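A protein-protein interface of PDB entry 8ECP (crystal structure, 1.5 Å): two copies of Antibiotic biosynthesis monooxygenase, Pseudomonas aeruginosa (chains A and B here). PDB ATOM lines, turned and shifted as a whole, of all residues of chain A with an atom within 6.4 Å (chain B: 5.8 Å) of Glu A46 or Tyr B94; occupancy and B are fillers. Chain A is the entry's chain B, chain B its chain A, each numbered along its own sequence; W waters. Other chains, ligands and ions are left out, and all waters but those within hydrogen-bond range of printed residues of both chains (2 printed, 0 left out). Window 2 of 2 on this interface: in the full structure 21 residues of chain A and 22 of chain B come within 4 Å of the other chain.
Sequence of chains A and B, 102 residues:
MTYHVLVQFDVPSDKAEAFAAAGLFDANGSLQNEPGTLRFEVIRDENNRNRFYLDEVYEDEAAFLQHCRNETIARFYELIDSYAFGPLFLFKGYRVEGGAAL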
ATOM      1  N   VAL A  42       0.116 -30.638   0.470  1.00  0.00           N
ATOM      2  CA  VAL A  42      -0.711 -29.863  -0.445  1.00  0.00           C
ATOM      3  C   VAL A  42       0.118 -29.609  -1.694  1.00  0.00           C
ATOM      4  O   VAL A  42       1.224 -29.070  -1.593  1.00  0.00           O
ATOM      5  CB  VAL A  42      -1.122 -28.527   0.197  1.00  0.00           C
ATOM      6  CG1 VAL A  42      -2.021 -27.742  -0.744  1.00  0.00           C
ATOM      7  CG2 VAL A  42      -1.780 -28.759   1.573  1.00  0.00           C
ATOM      8  N   ILE A  43      -0.409 -29.981  -2.861  1.00  0.00           N
ATOM      9  CA  ILE A  43       0.332 -29.903  -4.119  1.00  0.00           C
ATOM     10  C   ILE A  43      -0.478 -29.069  -5.106  1.00  0.00           C
ATOM     11  O   ILE A  43      -1.668 -29.330  -5.309  1.00  0.00           O
ATOM     12  CB  ILE A  43       0.617 -31.308  -4.688  1.00  0.00           C
ATOM     13  CG1 ILE A  43       1.492 -32.129  -3.738  1.00  0.00           C
ATOM     14  CG2 ILE A  43       1.285 -31.230  -6.049  1.00  0.00           C
ATOM     15  CD1 ILE A  43       1.337 -33.627  -3.927  1.00  0.00           C
ATOM     16  N   ARG A  44       0.157 -28.054  -5.708  1.00  0.00           N
ATOM     17  CA  ARG A  44      -0.477 -27.284  -6.779  1.00  0.00           C
ATOM     18  C   ARG A  44      -0.100 -27.858  -8.139  1.00  0.00           C
ATOM     19  O   ARG A  44       1.071 -28.160  -8.390  1.00  0.00           O
ATOM     20  CB  ARG A  44      -0.101 -25.802  -6.735  1.00  0.00           C
ATOM     21  CG  ARG A  44      -1.161 -24.966  -7.449  1.00  0.00           C
ATOM     22  CD  ARG A  44      -0.918 -23.468  -7.373  1.00  0.00           C
ATOM     23  NE  ARG A  44      -1.735 -22.757  -8.353  1.00  0.00           N
ATOM     24  CZ  ARG A  44      -1.962 -21.451  -8.336  1.00  0.00           C
ATOM     25  NH1 ARG A  44      -1.394 -20.662  -7.437  1.00  0.00           N
ATOM     26  NH2 ARG A  44      -2.773 -20.920  -9.248  1.00  0.00           N
ATOM     27  N   ASP A  45      -1.097 -28.034  -9.008  1.00  0.00           N
ATOM     28  CA  ASP A  45      -0.804 -28.492 -10.361  1.00  0.00           C
ATOM     29  C   ASP A  45       0.158 -27.523 -11.042  1.00  0.00           C
ATOM     30  O   ASP A  45       0.069 -26.306 -10.863  1.00  0.00           O
ATOM     31  CB  ASP A  45      -2.089 -28.595 -11.184  1.00  0.00           C
ATOM     32  CG  ASP A  45      -1.887 -29.383 -12.450  1.00  0.00           C
ATOM     33  OD1 ASP A  45      -1.483 -28.793 -13.467  1.00  0.00           O
ATOM     34  OD2 ASP A  45      -2.097 -30.611 -12.415  1.00  0.00           O
ATOM     35  N   GLU A  46       1.089 -28.076 -11.826  1.00  0.00           N
ATOM     36  CA  GLU A  46       2.116 -27.264 -12.468  1.00  0.00           C
ATOM     37  C   GLU A  46       1.565 -26.302 -13.515  1.00  0.00           C
ATOM     38  O   GLU A  46       2.215 -25.292 -13.797  1.00  0.00           O
ATOM     39  CB  GLU A  46       3.215 -28.154 -13.068  1.00  0.00           C
ATOM     40  CG  GLU A  46       2.761 -29.013 -14.250  1.00  0.00           C
ATOM     41  CD  GLU A  46       3.889 -29.811 -14.893  1.00  0.00           C
ATOM     42  OE1 GLU A  46       5.061 -29.662 -14.485  1.00  0.00           O
ATOM     43  OE2 GLU A  46       3.596 -30.558 -15.857  1.00  0.00           O
ATOM     44  N   ASN A  47       0.408 -26.576 -14.096  1.00  0.00           N
ATOM     45  CA  ASN A  47      -0.129 -25.732 -15.158  1.00  0.00           C
ATOM     46  C   ASN A  47      -1.590 -25.356 -14.967  1.00  0.00           C
ATOM     47  O   ASN A  47      -1.983 -24.257 -15.359  1.00  0.00           O
ATOM     48  CB  ASN A  47       0.044 -26.449 -16.498  1.00  0.00           C
ATOM     49  CG  ASN A  47       1.476 -26.416 -16.994  1.00  0.00           C
ATOM     50  OD1 ASN A  47       2.070 -27.453 -17.287  1.00  0.00           O
ATOM     51  ND2 ASN A  47       2.027 -25.214 -17.121  1.00  0.00           N
ATOM     52  N   ASN A  48      -2.405 -26.246 -14.405  1.00  0.00           N
ATOM     53  CA  ASN A  48      -3.811 -25.948 -14.173  1.00  0.00           C
ATOM     54  C   ASN A  48      -3.908 -24.958 -13.015  1.00  0.00           C
ATOM     55  O   ASN A  48      -3.549 -25.280 -11.878  1.00  0.00           O
ATOM     56  CB  ASN A  48      -4.552 -27.253 -13.876  1.00  0.00           C
ATOM     57  CG  ASN A  48      -6.075 -27.090 -13.866  1.00  0.00           C
ATOM     58  OD1 ASN A  48      -6.600 -26.037 -13.510  1.00  0.00           O
ATOM     59  ND2 ASN A  48      -6.784 -28.148 -14.242  1.00  0.00           N
ATOM     60  N   ARG A  51      -6.300 -26.142  -9.847  1.00  0.00           N
ATOM     61  CA  ARG A  51      -6.337 -27.496  -9.329  1.00  0.00           C
ATOM     62  C   ARG A  51      -5.236 -27.756  -8.316  1.00  0.00           C
ATOM     63  O   ARG A  51      -4.066 -27.428  -8.550  1.00  0.00           O
ATOM     64  CB  ARG A  51      -6.257 -28.503 -10.473  1.00  0.00           C
ATOM     65  CG  ARG A  51      -6.456 -29.937 -10.013  1.00  0.00           C
ATOM     66  CD  ARG A  51      -6.833 -30.843 -11.187  1.00  0.00           C
ATOM     67  NE  ARG A  51      -8.219 -30.599 -11.582  1.00  0.00           N
ATOM     68  CZ  ARG A  51      -8.863 -31.254 -12.537  1.00  0.00           C
ATOM     69  NH1 ARG A  51      -8.261 -32.177 -13.268  1.00  0.00           N
ATOM     70  NH2 ARG A  51     -10.148 -30.982 -12.754  1.00  0.00           N
ATOM     71  N   TYR A  53      -4.022 -30.836  -5.138  1.00  0.00           N
ATOM     72  CA  TYR A  53      -4.104 -32.218  -4.684  1.00  0.00           C
ATOM     73  C   TYR A  53      -3.637 -32.283  -3.244  1.00  0.00           C
ATOM     74  O   TYR A  53      -2.680 -31.608  -2.867  1.00  0.00           O
ATOM     75  CB  TYR A  53      -3.200 -33.115  -5.557  1.00  0.00           C
ATOM     76  CG  TYR A  53      -3.368 -32.846  -7.029  1.00  0.00           C
ATOM     77  CD1 TYR A  53      -4.401 -33.449  -7.747  1.00  0.00           C
ATOM     78  CD2 TYR A  53      -2.528 -31.966  -7.700  1.00  0.00           C
ATOM     79  CE1 TYR A  53      -4.572 -33.200  -9.103  1.00  0.00           C
ATOM     80  CE2 TYR A  53      -2.703 -31.699  -9.051  1.00  0.00           C
ATOM     81  CZ  TYR A  53      -3.729 -32.322  -9.742  1.00  0.00           C
ATOM     82  OH  TYR A  53      -3.896 -32.072 -11.089  1.00  0.00           O
ATOM     83  N   THR B   2       9.467 -28.848  -3.817  1.00  0.00           N
ATOM     84  CA  THR B   2       9.583 -30.181  -4.418  1.00  0.00           C
ATOM     85  C   THR B   2       8.574 -30.404  -5.538  1.00  0.00           C
ATOM     86  O   THR B   2       7.514 -29.782  -5.565  1.00  0.00           O
ATOM     87  CB  THR B   2       9.466 -31.312  -3.371  1.00  0.00           C
ATOM     88  OG1 THR B   2       8.321 -31.091  -2.545  1.00  0.00           O
ATOM     89  CG2 THR B   2      10.709 -31.353  -2.499  1.00  0.00           C
ATOM     90  N   TYR B   3       8.935 -31.292  -6.460  1.00  0.00           N
ATOM     91  CA  TYR B   3       8.160 -31.573  -7.662  1.00  0.00           C
ATOM     92  C   TYR B   3       7.607 -32.981  -7.542  1.00  0.00           C
ATOM     93  O   TYR B   3       8.370 -33.938  -7.370  1.00  0.00           O
ATOM     94  CB  TYR B   3       9.052 -31.441  -8.893  1.00  0.00           C
ATOM     95  CG  TYR B   3       8.362 -31.527 -10.227  1.00  0.00           C
ATOM     96  CD1 TYR B   3       7.475 -30.539 -10.655  1.00  0.00           C
ATOM     97  CD2 TYR B   3       8.626 -32.585 -11.085  1.00  0.00           C
ATOM     98  CE1 TYR B   3       6.862 -30.627 -11.905  1.00  0.00           C
ATOM     99  CE2 TYR B   3       8.025 -32.681 -12.329  1.00  0.00           C
ATOM    100  CZ  TYR B   3       7.153 -31.700 -12.732  1.00  0.00           C
ATOM    101  OH  TYR B   3       6.570 -31.816 -13.967  1.00  0.00           O
ATOM    102  N   HIS B   4       6.290 -33.097  -7.611  1.00  0.00           N
ATOM    103  CA  HIS B   4       5.579 -34.340  -7.343  1.00  0.00           C
ATOM    104  C   HIS B   4       4.927 -34.850  -8.619  1.00  0.00           C
ATOM    105  O   HIS B   4       4.253 -34.083  -9.317  1.00  0.00           O
ATOM    106  CB  HIS B   4       4.520 -34.085  -6.270  1.00  0.00           C
ATOM    107  CG  HIS B   4       5.101 -33.697  -4.951  1.00  0.00           C
ATOM    108  ND1 HIS B   4       4.926 -34.458  -3.815  1.00  0.00           N
ATOM    109  CD2 HIS B   4       5.906 -32.668  -4.598  1.00  0.00           C
ATOM    110  CE1 HIS B   4       5.567 -33.889  -2.809  1.00  0.00           C
ATOM    111  NE2 HIS B   4       6.176 -32.806  -3.260  1.00  0.00           N
ATOM    112  N   ASP B  60      13.143 -30.937  -8.175  1.00  0.00           N
ATOM    113  CA  ASP B  60      12.572 -29.965  -9.106  1.00  0.00           C
ATOM    114  C   ASP B  60      12.232 -30.713 -10.391  1.00  0.00           C
ATOM    115  O   ASP B  60      12.454 -31.923 -10.498  1.00  0.00           O
ATOM    116  CB  ASP B  60      13.503 -28.760  -9.319  1.00  0.00           C
ATOM    117  CG  ASP B  60      14.929 -29.151  -9.697  1.00  0.00           C
ATOM    118  OD1 ASP B  60      15.174 -30.272 -10.181  1.00  0.00           O
ATOM    119  OD2 ASP B  60      15.832 -28.313  -9.499  1.00  0.00           O
ATOM    120  N   GLU B  61      11.687 -29.988 -11.375  1.00  0.00           N
ATOM    121  CA  GLU B  61      11.316 -30.660 -12.616  1.00  0.00           C
ATOM    122  C   GLU B  61      12.535 -31.261 -13.307  1.00  0.00           C
ATOM    123  O   GLU B  61      12.454 -32.349 -13.887  1.00  0.00           O
ATOM    124  CB  GLU B  61      10.592 -29.712 -13.565  1.00  0.00           C
ATOM    125  CG  GLU B  61      10.161 -30.425 -14.843  1.00  0.00           C
ATOM    126  CD  GLU B  61       9.661 -29.491 -15.904  1.00  0.00           C
ATOM    127  OE1 GLU B  61       9.951 -28.287 -15.796  1.00  0.00           O
ATOM    128  OE2 GLU B  61       8.986 -29.967 -16.847  1.00  0.00           O
ATOM    129  N   LYS B  92       1.292 -33.696 -12.353  1.00  0.00           N
ATOM    130  CA  LYS B  92       2.626 -33.222 -12.018  1.00  0.00           C
ATOM    131  C   LYS B  92       2.445 -31.864 -11.360  1.00  0.00           C
ATOM    132  O   LYS B  92       1.678 -31.042 -11.862  1.00  0.00           O
ATOM    133  CB  LYS B  92       3.435 -33.073 -13.297  1.00  0.00           C
ATOM    134  CG  LYS B  92       3.654 -34.385 -14.056  1.00  0.00           C
ATOM    135  CD  LYS B  92       4.291 -34.142 -15.427  1.00  0.00           C
ATOM    136  CE  LYS B  92       4.001 -35.307 -16.368  1.00  0.00           C
ATOM    137  NZ  LYS B  92       4.472 -35.064 -17.761  1.00  0.00           N
ATOM    138  N   GLY B  93       3.137 -31.615 -10.247  1.00  0.00           N
ATOM    139  CA  GLY B  93       2.886 -30.363  -9.546  1.00  0.00           C
ATOM    140  C   GLY B  93       3.958 -30.075  -8.520  1.00  0.00           C
ATOM    141  O   GLY B  93       4.920 -30.830  -8.366  1.00  0.00           O
ATOM    142  N   TYR B  94       3.773 -28.966  -7.811  1.00  0.00           N
ATOM    143  CA  TYR B  94       4.757 -28.466  -6.853  1.00  0.00           C
ATOM    144  C   TYR B  94       4.127 -28.399  -5.470  1.00  0.00           C
ATOM    145  O   TYR B  94       3.004 -27.917  -5.313  1.00  0.00           O
ATOM    146  CB  TYR B  94       5.230 -27.064  -7.258  1.00  0.00           C
ATOM    147  CG  TYR B  94       6.044 -27.083  -8.521  1.00  0.00           C
ATOM    148  CD1 TYR B  94       7.403 -27.347  -8.488  1.00  0.00           C
ATOM    149  CD2 TYR B  94       5.450 -26.851  -9.753  1.00  0.00           C
ATOM    150  CE1 TYR B  94       8.157 -27.375  -9.647  1.00  0.00           C
ATOM    151  CE2 TYR B  94       6.198 -26.874 -10.925  1.00  0.00           C
ATOM    152  CZ  TYR B  94       7.552 -27.139 -10.864  1.00  0.00           C
ATOM    153  OH  TYR B  94       8.299 -27.169 -12.020  1.00  0.00           O
ATOM    154  N   ARG B  95       4.868 -28.857  -4.459  1.00  0.00           N
ATOM    155  CA  ARG B  95       4.350 -28.835  -3.101  1.00  0.00           C
ATOM    156  C   ARG B  95       4.323 -27.404  -2.576  1.00  0.00           C
ATOM    157  O   ARG B  95       5.232 -26.608  -2.844  1.00  0.00           O
ATOM    158  CB  ARG B  95       5.241 -29.701  -2.199  1.00  0.00           C
ATOM    159  CG  ARG B  95       4.747 -29.842  -0.759  1.00  0.00           C
ATOM    160  CD  ARG B  95       5.508 -30.913   0.034  1.00  0.00           C
ATOM    161  NE  ARG B  95       6.901 -30.533   0.216  1.00  0.00           N
ATOM    162  CZ  ARG B  95       7.865 -31.351   0.621  1.00  0.00           C
ATOM    163  NH1 ARG B  95       7.624 -32.621   0.901  1.00  0.00           N
ATOM    164  NH2 ARG B  95       9.101 -30.878   0.748  1.00  0.00           N
ATOM    165  N   VAL B  96       3.260 -27.066  -1.852  1.00  0.00           N
ATOM    166  CA  VAL B  96       3.193 -25.793  -1.139  1.00  0.00           C
ATOM    167  C   VAL B  96       4.026 -25.953   0.128  1.00  0.00           C
ATOM    168  O   VAL B  96       3.718 -26.797   0.978  1.00  0.00           O
ATOM    169  CB  VAL B  96       1.738 -25.439  -0.806  1.00  0.00           C
ATOM    170  CG1 VAL B  96       1.664 -24.097  -0.074  1.00  0.00           C
ATOM    171  CG2 VAL B  96       0.894 -25.420  -2.074  1.00  0.00           C
HETATM  172  O   HOH W   1      -0.798 -32.263 -14.002  1.00  0.00           O
HETATM  173  O   HOH W   2       2.424 -29.406   1.766  1.00  0.00           O
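The side-chain hydroxyl (OH) of Tyr B3 lies within hydrogen-bond range of the side-chain carboxylate (OE1) of Glu A46.
The backbone carbonyl oxygen of Lys B92 is in hydrogen-bond range of the backbone NH of Glu A46 (3.0 Å).
The backbone carbonyl oxygen (O) of Val A42 is in hydrogen-bond range of the backbone NH (N) of Val B96 (2.9 Å).
The backbone NH of Arg A44 is in hydrogen-bond range of the backbone carbonyl oxygen of Tyr B94.
OD1 of Asp A45 is in hydrogen-bond range of N of Asn A47 (3.0 Å).
The backbone NH (N) of Ile A43 lies within hydrogen-bond range of the backbone carbonyl oxygen (O) of Tyr A53 (2.8 Å).
The side-chain hydroxyl (OH) of Tyr A53 is in hydrogen-bond range of the side-chain carboxylate (OD2) of Asp A45 (2.7 Å).
OD1 of Asp A45 sits at hydrogen-bond distance from N of Asn A48.
The backbone NH (N) of Arg B95 lies within hydrogen-bond range of the backbone carbonyl oxygen (O) of Thr B2, 3.0 Å away.
The backbone NH (N) of Asp A45 lies within hydrogen-bond range of the backbone carbonyl oxygen (O) of Arg A51.
Arg B95 touches Val A42.
His B4 touches Ile A43.
Gly B93 touches Ile A43.
Tyr B94 touches Ile A43.
Arg A44 touches Gly B93.
Asp A45 touches Lys B92.
N of Glu A46 touches CA of Gly B93 (3.7 Å).
CB of Glu A46 touches CE2 of Tyr B94 (3.9 Å).
Of the printed residues of chain A, Tyr B94 touches Ile A43 (3.5 Å), Arg A44 (2.9 Å) and Glu A46 (3.9 Å).
Of the printed residues of chain A, Tyr B3 touches Glu A46 (2.7 Å).
Of the printed residues of chain A, Arg B95 touches Val A42 (3.5 Å).
Of the printed residues of chain A, His B4 touches Ile A43 (3.7 Å).
Of the printed residues of chain B, Arg A44 touches Gly B93 and Tyr B94.
Of the printed residues of chain A, Val B96 touches Val A42 (2.9 Å).
Thr B2 touches none of the printed residues of chain A.
Asp B60 touches none of the printed residues of chain A.
The nearest residue of chain B that does not touch Glu A46 is Glu B61 (4.6 Å).
Of the 9 printed residues of chain A, 5 touch a printed residue of chain B.
Printed residues of chain A that touch a printed residue of chain B: Val A42, Ile A43, Arg A44, Asp A45 and Glu A46.
Along chain B the printed residues that touch a printed residue of chain A span positions 3 to 96.
Among the printed residues, no Asp or Glu carboxylate lies within 4 Å of a Lys or Arg side-chain nitrogen of the other chain.
No position is printed for both chains.
Water W1 lies within hydrogen-bond range of OD2 of Asp A45 (2.6 Å) and N of Lys B92 (3.0 Å).
Water W2 lies within hydrogen-bond range of the backbone NH of Val A42 (2.9 Å) and the backbone carbonyl oxygen of Val B96 (3.0 Å).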
